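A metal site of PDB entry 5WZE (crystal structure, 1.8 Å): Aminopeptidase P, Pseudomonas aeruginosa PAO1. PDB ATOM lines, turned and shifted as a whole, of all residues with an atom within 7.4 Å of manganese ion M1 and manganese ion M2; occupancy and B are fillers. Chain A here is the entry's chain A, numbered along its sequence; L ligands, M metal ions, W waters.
O1 of the ligand sits close to NE2 of His 361, 3.3 Å away.
NE2 of His 243 is in hydrogen-bond range of N1 of the ligand, 2.8 Å away.
The side-chain carboxylate (OE2) of Glu 384 sits close to the side-chain hydroxyl (OG1) of Thr 382, at 2.8 Å.
The backbone NH of Ile 232 is in hydrogen-bond range of the backbone carbonyl oxygen of Asp 260 (2.9 Å).
N of Glu 384 sits at hydrogen-bond distance from O of Ala 352, 2.7 Å away.
OH of Tyr 229 sits at hydrogen-bond distance from N of Gly 262 (3.4 Å).
The backbone NH of Asp 271 lies within hydrogen-bond range of the side-chain carboxylate of Asp 410, 2.8 Å away.
O of Thr 273 lies within hydrogen-bond range of N of Glu 408 (3.0 Å).
OD2 of Asp 260 sits close to OG1 of Thr 273.
A ring nitrogen (ND1) of His 354 lies close to the backbone carbonyl oxygen (O) of Val 360, at 3.0 Å.
Merely in contact with manganese ion M1: Thr 382.
Along chain A the residues within 4 Å of manganese ion M1 span positions 271 to 408.
Tyr 229 touches manganese ion M2 (OH to MN, 3.6 Å).
OG1 of Thr 273 touches manganese ion M2, at 3.6 Å.
Six residues have an atom within 4 Å of manganese ion M2: Tyr 229, Asp 260, Asp 271, Thr 273, Glu 384 and Glu 408.
The nearest printed residue that does not touch manganese ion M2 is Ile 272 (4.5 Å).
Manganese ion M1 is bound by OE2 of Glu 408, water W1, OD2 of Asp 271, NE2 of His 354 and OE2 of Glu 384.
Slightly farther from manganese ion M1 lies OE1 of Glu 384 (2.9 Å).
Manganese ion M2 is bound by OD1 of Asp 271, OE1 of Glu 408, OD1 of Asp 260, water W1 and OD2 of Asp 260.
Manganese ion M2 has five donor atoms within binding distance.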
ATOM      1  N   TYR A 229     -17.006 -10.479 -25.868  1.00  0.00           N
ATOM      2  CA  TYR A 229     -18.259 -10.656 -25.149  1.00  0.00           C
ATOM      3  C   TYR A 229     -18.091  -9.954 -23.810  1.00  0.00           C
ATOM      4  O   TYR A 229     -16.967  -9.664 -23.388  1.00  0.00           O
ATOM      5  CB  TYR A 229     -18.610 -12.139 -24.973  1.00  0.00           C
ATOM      6  CG  TYR A 229     -17.474 -12.965 -24.396  1.00  0.00           C
ATOM      7  CD1 TYR A 229     -16.493 -13.504 -25.215  1.00  0.00           C
ATOM      8  CD2 TYR A 229     -17.382 -13.194 -23.041  1.00  0.00           C
ATOM      9  CE1 TYR A 229     -15.473 -14.245 -24.694  1.00  0.00           C
ATOM     10  CE2 TYR A 229     -16.362 -13.943 -22.515  1.00  0.00           C
ATOM     11  CZ  TYR A 229     -15.402 -14.464 -23.343  1.00  0.00           C
ATOM     12  OH  TYR A 229     -14.369 -15.208 -22.827  1.00  0.00           O
ATOM     13  N   ILE A 232     -17.087 -11.922 -17.730  1.00  0.00           N
ATOM     14  CA  ILE A 232     -17.666 -12.536 -16.551  1.00  0.00           C
ATOM     15  C   ILE A 232     -16.602 -12.592 -15.466  1.00  0.00           C
ATOM     16  O   ILE A 232     -15.563 -13.226 -15.642  1.00  0.00           O
ATOM     17  CB  ILE A 232     -18.185 -13.949 -16.882  1.00  0.00           C
ATOM     18  CG1 ILE A 232     -19.368 -13.836 -17.850  1.00  0.00           C
ATOM     19  CG2 ILE A 232     -18.507 -14.715 -15.616  1.00  0.00           C
ATOM     20  CD1 ILE A 232     -19.609 -15.052 -18.596  1.00  0.00           C
ATOM     21  N   HIS A 243     -23.274 -17.139 -16.820  1.00  0.00           N
ATOM     22  CA  HIS A 243     -22.964 -15.880 -17.503  1.00  0.00           C
ATOM     23  C   HIS A 243     -23.167 -14.686 -16.571  1.00  0.00           C
ATOM     24  O   HIS A 243     -23.724 -13.665 -16.971  1.00  0.00           O
ATOM     25  CB  HIS A 243     -23.850 -15.686 -18.735  1.00  0.00           C
ATOM     26  CG  HIS A 243     -23.502 -16.586 -19.871  1.00  0.00           C
ATOM     27  ND1 HIS A 243     -24.319 -16.750 -20.970  1.00  0.00           N
ATOM     28  CD2 HIS A 243     -22.434 -17.394 -20.070  1.00  0.00           C
ATOM     29  CE1 HIS A 243     -23.763 -17.605 -21.804  1.00  0.00           C
ATOM     30  NE2 HIS A 243     -22.624 -18.010 -21.283  1.00  0.00           N
ATOM     31  N   ILE A 259     -13.158 -16.302 -14.017  1.00  0.00           N
ATOM     32  CA  ILE A 259     -13.088 -15.214 -14.993  1.00  0.00           C
ATOM     33  C   ILE A 259     -13.211 -15.794 -16.383  1.00  0.00           C
ATOM     34  O   ILE A 259     -12.324 -16.522 -16.842  1.00  0.00           O
ATOM     35  CB  ILE A 259     -11.781 -14.411 -14.898  1.00  0.00           C
ATOM     36  CG1 ILE A 259     -11.676 -13.709 -13.560  1.00  0.00           C
ATOM     37  CG2 ILE A 259     -11.734 -13.355 -16.029  1.00  0.00           C
ATOM     38  CD1 ILE A 259     -10.547 -12.745 -13.535  1.00  0.00           C
ATOM     39  N   ASP A 260     -14.279 -15.434 -17.074  1.00  0.00           N
ATOM     40  CA  ASP A 260     -14.513 -15.836 -18.454  1.00  0.00           C
ATOM     41  C   ASP A 260     -14.481 -14.560 -19.280  1.00  0.00           C
ATOM     42  O   ASP A 260     -15.379 -13.729 -19.167  1.00  0.00           O
ATOM     43  CB  ASP A 260     -15.853 -16.568 -18.588  1.00  0.00           C
ATOM     44  CG  ASP A 260     -16.056 -17.215 -19.953  1.00  0.00           C
ATOM     45  OD1 ASP A 260     -15.407 -16.800 -20.927  1.00  0.00           O
ATOM     46  OD2 ASP A 260     -16.841 -18.164 -20.073  1.00  0.00           O
ATOM     47  N   ALA A 261     -13.434 -14.388 -20.084  1.00  0.00           N
ATOM     48  CA  ALA A 261     -13.250 -13.128 -20.769  1.00  0.00           C
ATOM     49  C   ALA A 261     -12.280 -13.318 -21.911  1.00  0.00           C
ATOM     50  O   ALA A 261     -11.442 -14.213 -21.889  1.00  0.00           O
ATOM     51  CB  ALA A 261     -12.752 -12.048 -19.808  1.00  0.00           C
ATOM     52  N   GLY A 262     -12.419 -12.470 -22.926  1.00  0.00           N
ATOM     53  CA  GLY A 262     -11.580 -12.531 -24.096  1.00  0.00           C
ATOM     54  C   GLY A 262     -11.775 -11.313 -24.978  1.00  0.00           C
ATOM     55  O   GLY A 262     -12.899 -10.838 -25.129  1.00  0.00           O
ATOM     56  N   SER A 270     -11.414 -14.243 -29.152  1.00  0.00           N
ATOM     57  CA  SER A 270     -10.772 -15.241 -28.307  1.00  0.00           C
ATOM     58  C   SER A 270     -11.682 -15.430 -27.098  1.00  0.00           C
ATOM     59  O   SER A 270     -12.564 -14.616 -26.851  1.00  0.00           O
ATOM     60  CB  SER A 270      -9.378 -14.816 -27.876  1.00  0.00           C
ATOM     61  OG  SER A 270      -9.501 -13.709 -27.017  1.00  0.00           O
ATOM     62  N   ASP A 271     -11.484 -16.525 -26.338  1.00  0.00           N
ATOM     63  CA  ASP A 271     -12.453 -16.932 -25.327  1.00  0.00           C
ATOM     64  C   ASP A 271     -11.723 -17.800 -24.289  1.00  0.00           C
ATOM     65  O   ASP A 271     -11.405 -18.944 -24.575  1.00  0.00           O
ATOM     66  CB  ASP A 271     -13.611 -17.660 -26.002  1.00  0.00           C
ATOM     67  CG  ASP A 271     -14.747 -18.045 -25.051  1.00  0.00           C
ATOM     68  OD1 ASP A 271     -14.606 -17.902 -23.841  1.00  0.00           O
ATOM     69  OD2 ASP A 271     -15.797 -18.489 -25.554  1.00  0.00           O
ATOM     70  N   ILE A 272     -11.460 -17.242 -23.106  1.00  0.00           N
ATOM     71  CA  ILE A 272     -10.672 -17.906 -22.069  1.00  0.00           C
ATOM     72  C   ILE A 272     -11.419 -17.840 -20.748  1.00  0.00           C
ATOM     73  O   ILE A 272     -11.921 -16.792 -20.358  1.00  0.00           O
ATOM     74  CB  ILE A 272      -9.279 -17.268 -21.875  1.00  0.00           C
ATOM     75  CG1 ILE A 272      -8.398 -17.397 -23.108  1.00  0.00           C
ATOM     76  CG2 ILE A 272      -8.555 -17.897 -20.682  1.00  0.00           C
ATOM     77  CD1 ILE A 272      -7.062 -16.685 -22.950  1.00  0.00           C
ATOM     78  N   THR A 273     -11.467 -18.963 -20.034  1.00  0.00           N
ATOM     79  CA  THR A 273     -11.897 -19.003 -18.646  1.00  0.00           C
ATOM     80  C   THR A 273     -10.779 -19.596 -17.799  1.00  0.00           C
ATOM     81  O   THR A 273     -10.196 -20.624 -18.156  1.00  0.00           O
ATOM     82  CB  THR A 273     -13.176 -19.817 -18.438  1.00  0.00           C
ATOM     83  OG1 THR A 273     -14.222 -19.306 -19.262  1.00  0.00           O
ATOM     84  CG2 THR A 273     -13.616 -19.746 -16.977  1.00  0.00           C
ATOM     85  N   ALA A 352     -19.420 -28.695 -23.746  1.00  0.00           N
ATOM     86  CA  ALA A 352     -17.984 -28.542 -23.572  1.00  0.00           C
ATOM     87  C   ALA A 352     -17.362 -27.549 -24.531  1.00  0.00           C
ATOM     88  O   ALA A 352     -16.152 -27.294 -24.408  1.00  0.00           O
ATOM     89  CB  ALA A 352     -17.289 -29.896 -23.747  1.00  0.00           C
ATOM     90  N   GLY A 353     -18.114 -26.994 -25.478  1.00  0.00           N
ATOM     91  CA  GLY A 353     -17.525 -26.024 -26.383  1.00  0.00           C
ATOM     92  C   GLY A 353     -18.444 -25.606 -27.500  1.00  0.00           C
ATOM     93  O   GLY A 353     -19.614 -26.018 -27.587  1.00  0.00           O
ATOM     94  N   HIS A 354     -17.890 -24.773 -28.377  1.00  0.00           N
ATOM     95  CA  HIS A 354     -18.607 -24.182 -29.502  1.00  0.00           C
ATOM     96  C   HIS A 354     -17.595 -23.766 -30.552  1.00  0.00           C
ATOM     97  O   HIS A 354     -16.412 -23.597 -30.254  1.00  0.00           O
ATOM     98  CB  HIS A 354     -19.448 -23.001 -29.052  1.00  0.00           C
ATOM     99  CG  HIS A 354     -18.704 -21.996 -28.229  1.00  0.00           C
ATOM    100  ND1 HIS A 354     -17.856 -21.052 -28.774  1.00  0.00           N
ATOM    101  CD2 HIS A 354     -18.679 -21.775 -26.890  1.00  0.00           C
ATOM    102  CE1 HIS A 354     -17.338 -20.312 -27.814  1.00  0.00           C
ATOM    103  NE2 HIS A 354     -17.817 -20.738 -26.657  1.00  0.00           N
ATOM    104  N   TRP A 355     -18.057 -23.611 -31.796  1.00  0.00           N
ATOM    105  CA  TRP A 355     -17.182 -23.035 -32.809  1.00  0.00           C
ATOM    106  C   TRP A 355     -16.704 -21.658 -32.355  1.00  0.00           C
ATOM    107  O   TRP A 355     -17.379 -20.967 -31.588  1.00  0.00           O
ATOM    108  CB  TRP A 355     -17.889 -22.892 -34.148  1.00  0.00           C
ATOM    109  CG  TRP A 355     -18.528 -24.119 -34.761  1.00  0.00           C
ATOM    110  CD1 TRP A 355     -19.843 -24.271 -35.089  1.00  0.00           C
ATOM    111  CD2 TRP A 355     -17.878 -25.331 -35.155  1.00  0.00           C
ATOM    112  NE1 TRP A 355     -20.053 -25.503 -35.644  1.00  0.00           N
ATOM    113  CE2 TRP A 355     -18.862 -26.171 -35.705  1.00  0.00           C
ATOM    114  CE3 TRP A 355     -16.568 -25.791 -35.103  1.00  0.00           C
ATOM    115  CZ2 TRP A 355     -18.577 -27.446 -36.185  1.00  0.00           C
ATOM    116  CZ3 TRP A 355     -16.280 -27.046 -35.570  1.00  0.00           C
ATOM    117  CH2 TRP A 355     -17.283 -27.863 -36.105  1.00  0.00           C
ATOM    118  N   LEU A 356     -15.540 -21.260 -32.841  1.00  0.00           N
ATOM    119  CA  LEU A 356     -14.921 -20.000 -32.465  1.00  0.00           C
ATOM    120  C   LEU A 356     -14.480 -19.266 -33.721  1.00  0.00           C
ATOM    121  O   LEU A 356     -13.864 -19.851 -34.600  1.00  0.00           O
ATOM    122  CB  LEU A 356     -13.721 -20.208 -31.565  1.00  0.00           C
ATOM    123  CG  LEU A 356     -13.063 -18.970 -30.953  1.00  0.00           C
ATOM    124  CD1 LEU A 356     -13.990 -18.280 -29.983  1.00  0.00           C
ATOM    125  CD2 LEU A 356     -11.786 -19.369 -30.261  1.00  0.00           C
ATOM    126  N   VAL A 360     -18.093 -15.062 -31.195  1.00  0.00           N
ATOM    127  CA  VAL A 360     -17.476 -15.943 -30.197  1.00  0.00           C
ATOM    128  C   VAL A 360     -18.157 -17.315 -30.187  1.00  0.00           C
ATOM    129  O   VAL A 360     -17.495 -18.343 -30.098  1.00  0.00           O
ATOM    130  CB  VAL A 360     -17.476 -15.274 -28.804  1.00  0.00           C
ATOM    131  CG1 VAL A 360     -18.861 -14.973 -28.329  1.00  0.00           C
ATOM    132  CG2 VAL A 360     -16.713 -16.118 -27.820  1.00  0.00           C
ATOM    133  N   HIS A 361     -19.466 -17.367 -30.388  1.00  0.00           N
ATOM    134  CA  HIS A 361     -20.183 -18.647 -30.637  1.00  0.00           C
ATOM    135  C   HIS A 361     -20.316 -18.582 -32.180  1.00  0.00           C
ATOM    136  O   HIS A 361     -21.248 -18.042 -32.692  1.00  0.00           O
ATOM    137  CB  HIS A 361     -21.536 -18.714 -29.972  1.00  0.00           C
ATOM    138  CG  HIS A 361     -21.454 -18.679 -28.495  1.00  0.00           C
ATOM    139  ND1 HIS A 361     -22.470 -18.220 -27.687  1.00  0.00           N
ATOM    140  CD2 HIS A 361     -20.462 -19.027 -27.664  1.00  0.00           C
ATOM    141  CE1 HIS A 361     -22.100 -18.294 -26.435  1.00  0.00           C
ATOM    142  NE2 HIS A 361     -20.878 -18.773 -26.395  1.00  0.00           N
ATOM    143  N   THR A 382     -13.786 -24.045 -28.902  1.00  0.00           N
ATOM    144  CA  THR A 382     -13.406 -23.949 -27.506  1.00  0.00           C
ATOM    145  C   THR A 382     -13.555 -25.316 -26.835  1.00  0.00           C
ATOM    146  O   THR A 382     -14.208 -26.232 -27.346  1.00  0.00           O
ATOM    147  CB  THR A 382     -14.267 -22.924 -26.752  1.00  0.00           C
ATOM    148  OG1 THR A 382     -15.648 -23.335 -26.736  1.00  0.00           O
ATOM    149  CG2 THR A 382     -14.113 -21.557 -27.369  1.00  0.00           C
ATOM    150  N   VAL A 383     -12.904 -25.435 -25.677  1.00  0.00           N
ATOM    151  CA  VAL A 383     -12.988 -26.568 -24.767  1.00  0.00           C
ATOM    152  C   VAL A 383     -13.172 -25.985 -23.381  1.00  0.00           C
ATOM    153  O   VAL A 383     -12.261 -25.334 -22.861  1.00  0.00           O
ATOM    154  CB  VAL A 383     -11.709 -27.412 -24.798  1.00  0.00           C
ATOM    155  CG1 VAL A 383     -11.700 -28.398 -23.652  1.00  0.00           C
ATOM    156  CG2 VAL A 383     -11.531 -28.080 -26.115  1.00  0.00           C
ATOM    157  N   GLU A 384     -14.341 -26.189 -22.787  1.00  0.00           N
ATOM    158  CA  GLU A 384     -14.600 -25.491 -21.538  1.00  0.00           C
ATOM    159  C   GLU A 384     -15.438 -26.307 -20.536  1.00  0.00           C
ATOM    160  O   GLU A 384     -16.508 -25.870 -20.136  1.00  0.00           O
ATOM    161  CB  GLU A 384     -15.291 -24.152 -21.828  1.00  0.00           C
ATOM    162  CG  GLU A 384     -16.508 -24.248 -22.731  1.00  0.00           C
ATOM    163  CD  GLU A 384     -17.006 -22.881 -23.189  1.00  0.00           C
ATOM    164  OE1 GLU A 384     -17.243 -22.006 -22.336  1.00  0.00           O
ATOM    165  OE2 GLU A 384     -17.133 -22.690 -24.405  1.00  0.00           O
ATOM    166  N   ARG A 406     -14.515 -23.452 -13.949  1.00  0.00           N
ATOM    167  CA  ARG A 406     -14.496 -23.683 -15.390  1.00  0.00           C
ATOM    168  C   ARG A 406     -13.108 -23.367 -15.903  1.00  0.00           C
ATOM    169  O   ARG A 406     -12.494 -22.388 -15.478  1.00  0.00           O
ATOM    170  CB  ARG A 406     -15.550 -22.837 -16.113  1.00  0.00           C
ATOM    171  CG  ARG A 406     -15.473 -22.950 -17.611  1.00  0.00           C
ATOM    172  CD  ARG A 406     -16.810 -22.554 -18.275  1.00  0.00           C
ATOM    173  NE  ARG A 406     -17.041 -21.102 -18.368  1.00  0.00           N
ATOM    174  CZ  ARG A 406     -17.875 -20.451 -17.577  1.00  0.00           C
ATOM    175  NH1 ARG A 406     -18.525 -21.103 -16.633  1.00  0.00           N
ATOM    176  NH2 ARG A 406     -18.057 -19.145 -17.742  1.00  0.00           N
ATOM    177  N   GLU A 408     -11.206 -23.017 -19.604  1.00  0.00           N
ATOM    178  CA  GLU A 408     -11.519 -22.916 -21.029  1.00  0.00           C
ATOM    179  C   GLU A 408     -10.310 -22.540 -21.865  1.00  0.00           C
ATOM    180  O   GLU A 408      -9.586 -21.593 -21.539  1.00  0.00           O
ATOM    181  CB  GLU A 408     -12.633 -21.888 -21.273  1.00  0.00           C
ATOM    182  CG  GLU A 408     -12.931 -21.607 -22.752  1.00  0.00           C
ATOM    183  CD  GLU A 408     -14.204 -20.780 -22.976  1.00  0.00           C
ATOM    184  OE1 GLU A 408     -14.653 -20.074 -22.057  1.00  0.00           O
ATOM    185  OE2 GLU A 408     -14.771 -20.847 -24.086  1.00  0.00           O
ATOM    186  N   ASP A 409     -10.101 -23.249 -22.974  1.00  0.00           N
ATOM    187  CA  ASP A 409      -9.076 -22.932 -23.938  1.00  0.00           C
ATOM    188  C   ASP A 409      -9.658 -22.838 -25.345  1.00  0.00           C
ATOM    189  O   ASP A 409     -10.757 -23.322 -25.623  1.00  0.00           O
ATOM    190  CB  ASP A 409      -7.960 -23.954 -23.917  1.00  0.00           C
ATOM    191  CG  ASP A 409      -7.152 -23.868 -22.666  1.00  0.00           C
ATOM    192  OD1 ASP A 409      -6.505 -22.832 -22.459  1.00  0.00           O
ATOM    193  OD2 ASP A 409      -7.202 -24.836 -21.867  1.00  0.00           O
ATOM    194  N   ASP A 410      -8.896 -22.198 -26.232  1.00  0.00           N
ATOM    195  CA  ASP A 410      -9.256 -22.096 -27.640  1.00  0.00           C
ATOM    196  C   ASP A 410      -8.317 -22.950 -28.479  1.00  0.00           C
ATOM    197  O   ASP A 410      -7.118 -23.019 -28.228  1.00  0.00           O
ATOM    198  CB  ASP A 410      -9.203 -20.643 -28.115  1.00  0.00           C
ATOM    199  CG  ASP A 410     -10.038 -19.736 -27.268  1.00  0.00           C
ATOM    200  OD1 ASP A 410     -11.014 -20.225 -26.680  1.00  0.00           O
ATOM    201  OD2 ASP A 410      -9.694 -18.541 -27.172  1.00  0.00           O
HETATM  202  N1  LIG L   1     -20.988 -20.281 -21.235  1.00  0.00           N
HETATM  203  C1  LIG L   1     -21.174 -20.981 -22.519  1.00  0.00           C
HETATM  204  C2  LIG L   1     -22.553 -20.714 -23.176  1.00  0.00           C
HETATM  205  O1  LIG L   1     -22.748 -20.625 -24.349  1.00  0.00           O
HETATM  206  C3  LIG L   1     -20.994 -22.446 -22.142  1.00  0.00           C
HETATM  207  C4  LIG L   1     -20.334 -22.445 -20.806  1.00  0.00           C
HETATM  208  C5  LIG L   1     -20.734 -21.213 -20.126  1.00  0.00           C
HETATM  209  O2  LIG L   1     -23.597 -20.609 -22.587  1.00  0.00           O
HETATM  210 MN    MN M   1     -16.725 -20.383 -24.647  1.00  0.00          MN
HETATM  211 MN    MN M   2     -15.735 -18.469 -22.376  1.00  0.00          MN
HETATM  212 MN    MN M   3     -18.766 -17.578 -23.460  1.00  0.00          MN
HETATM  213  O   HOH W   1     -17.783 -19.440 -23.006  1.00  0.00           O
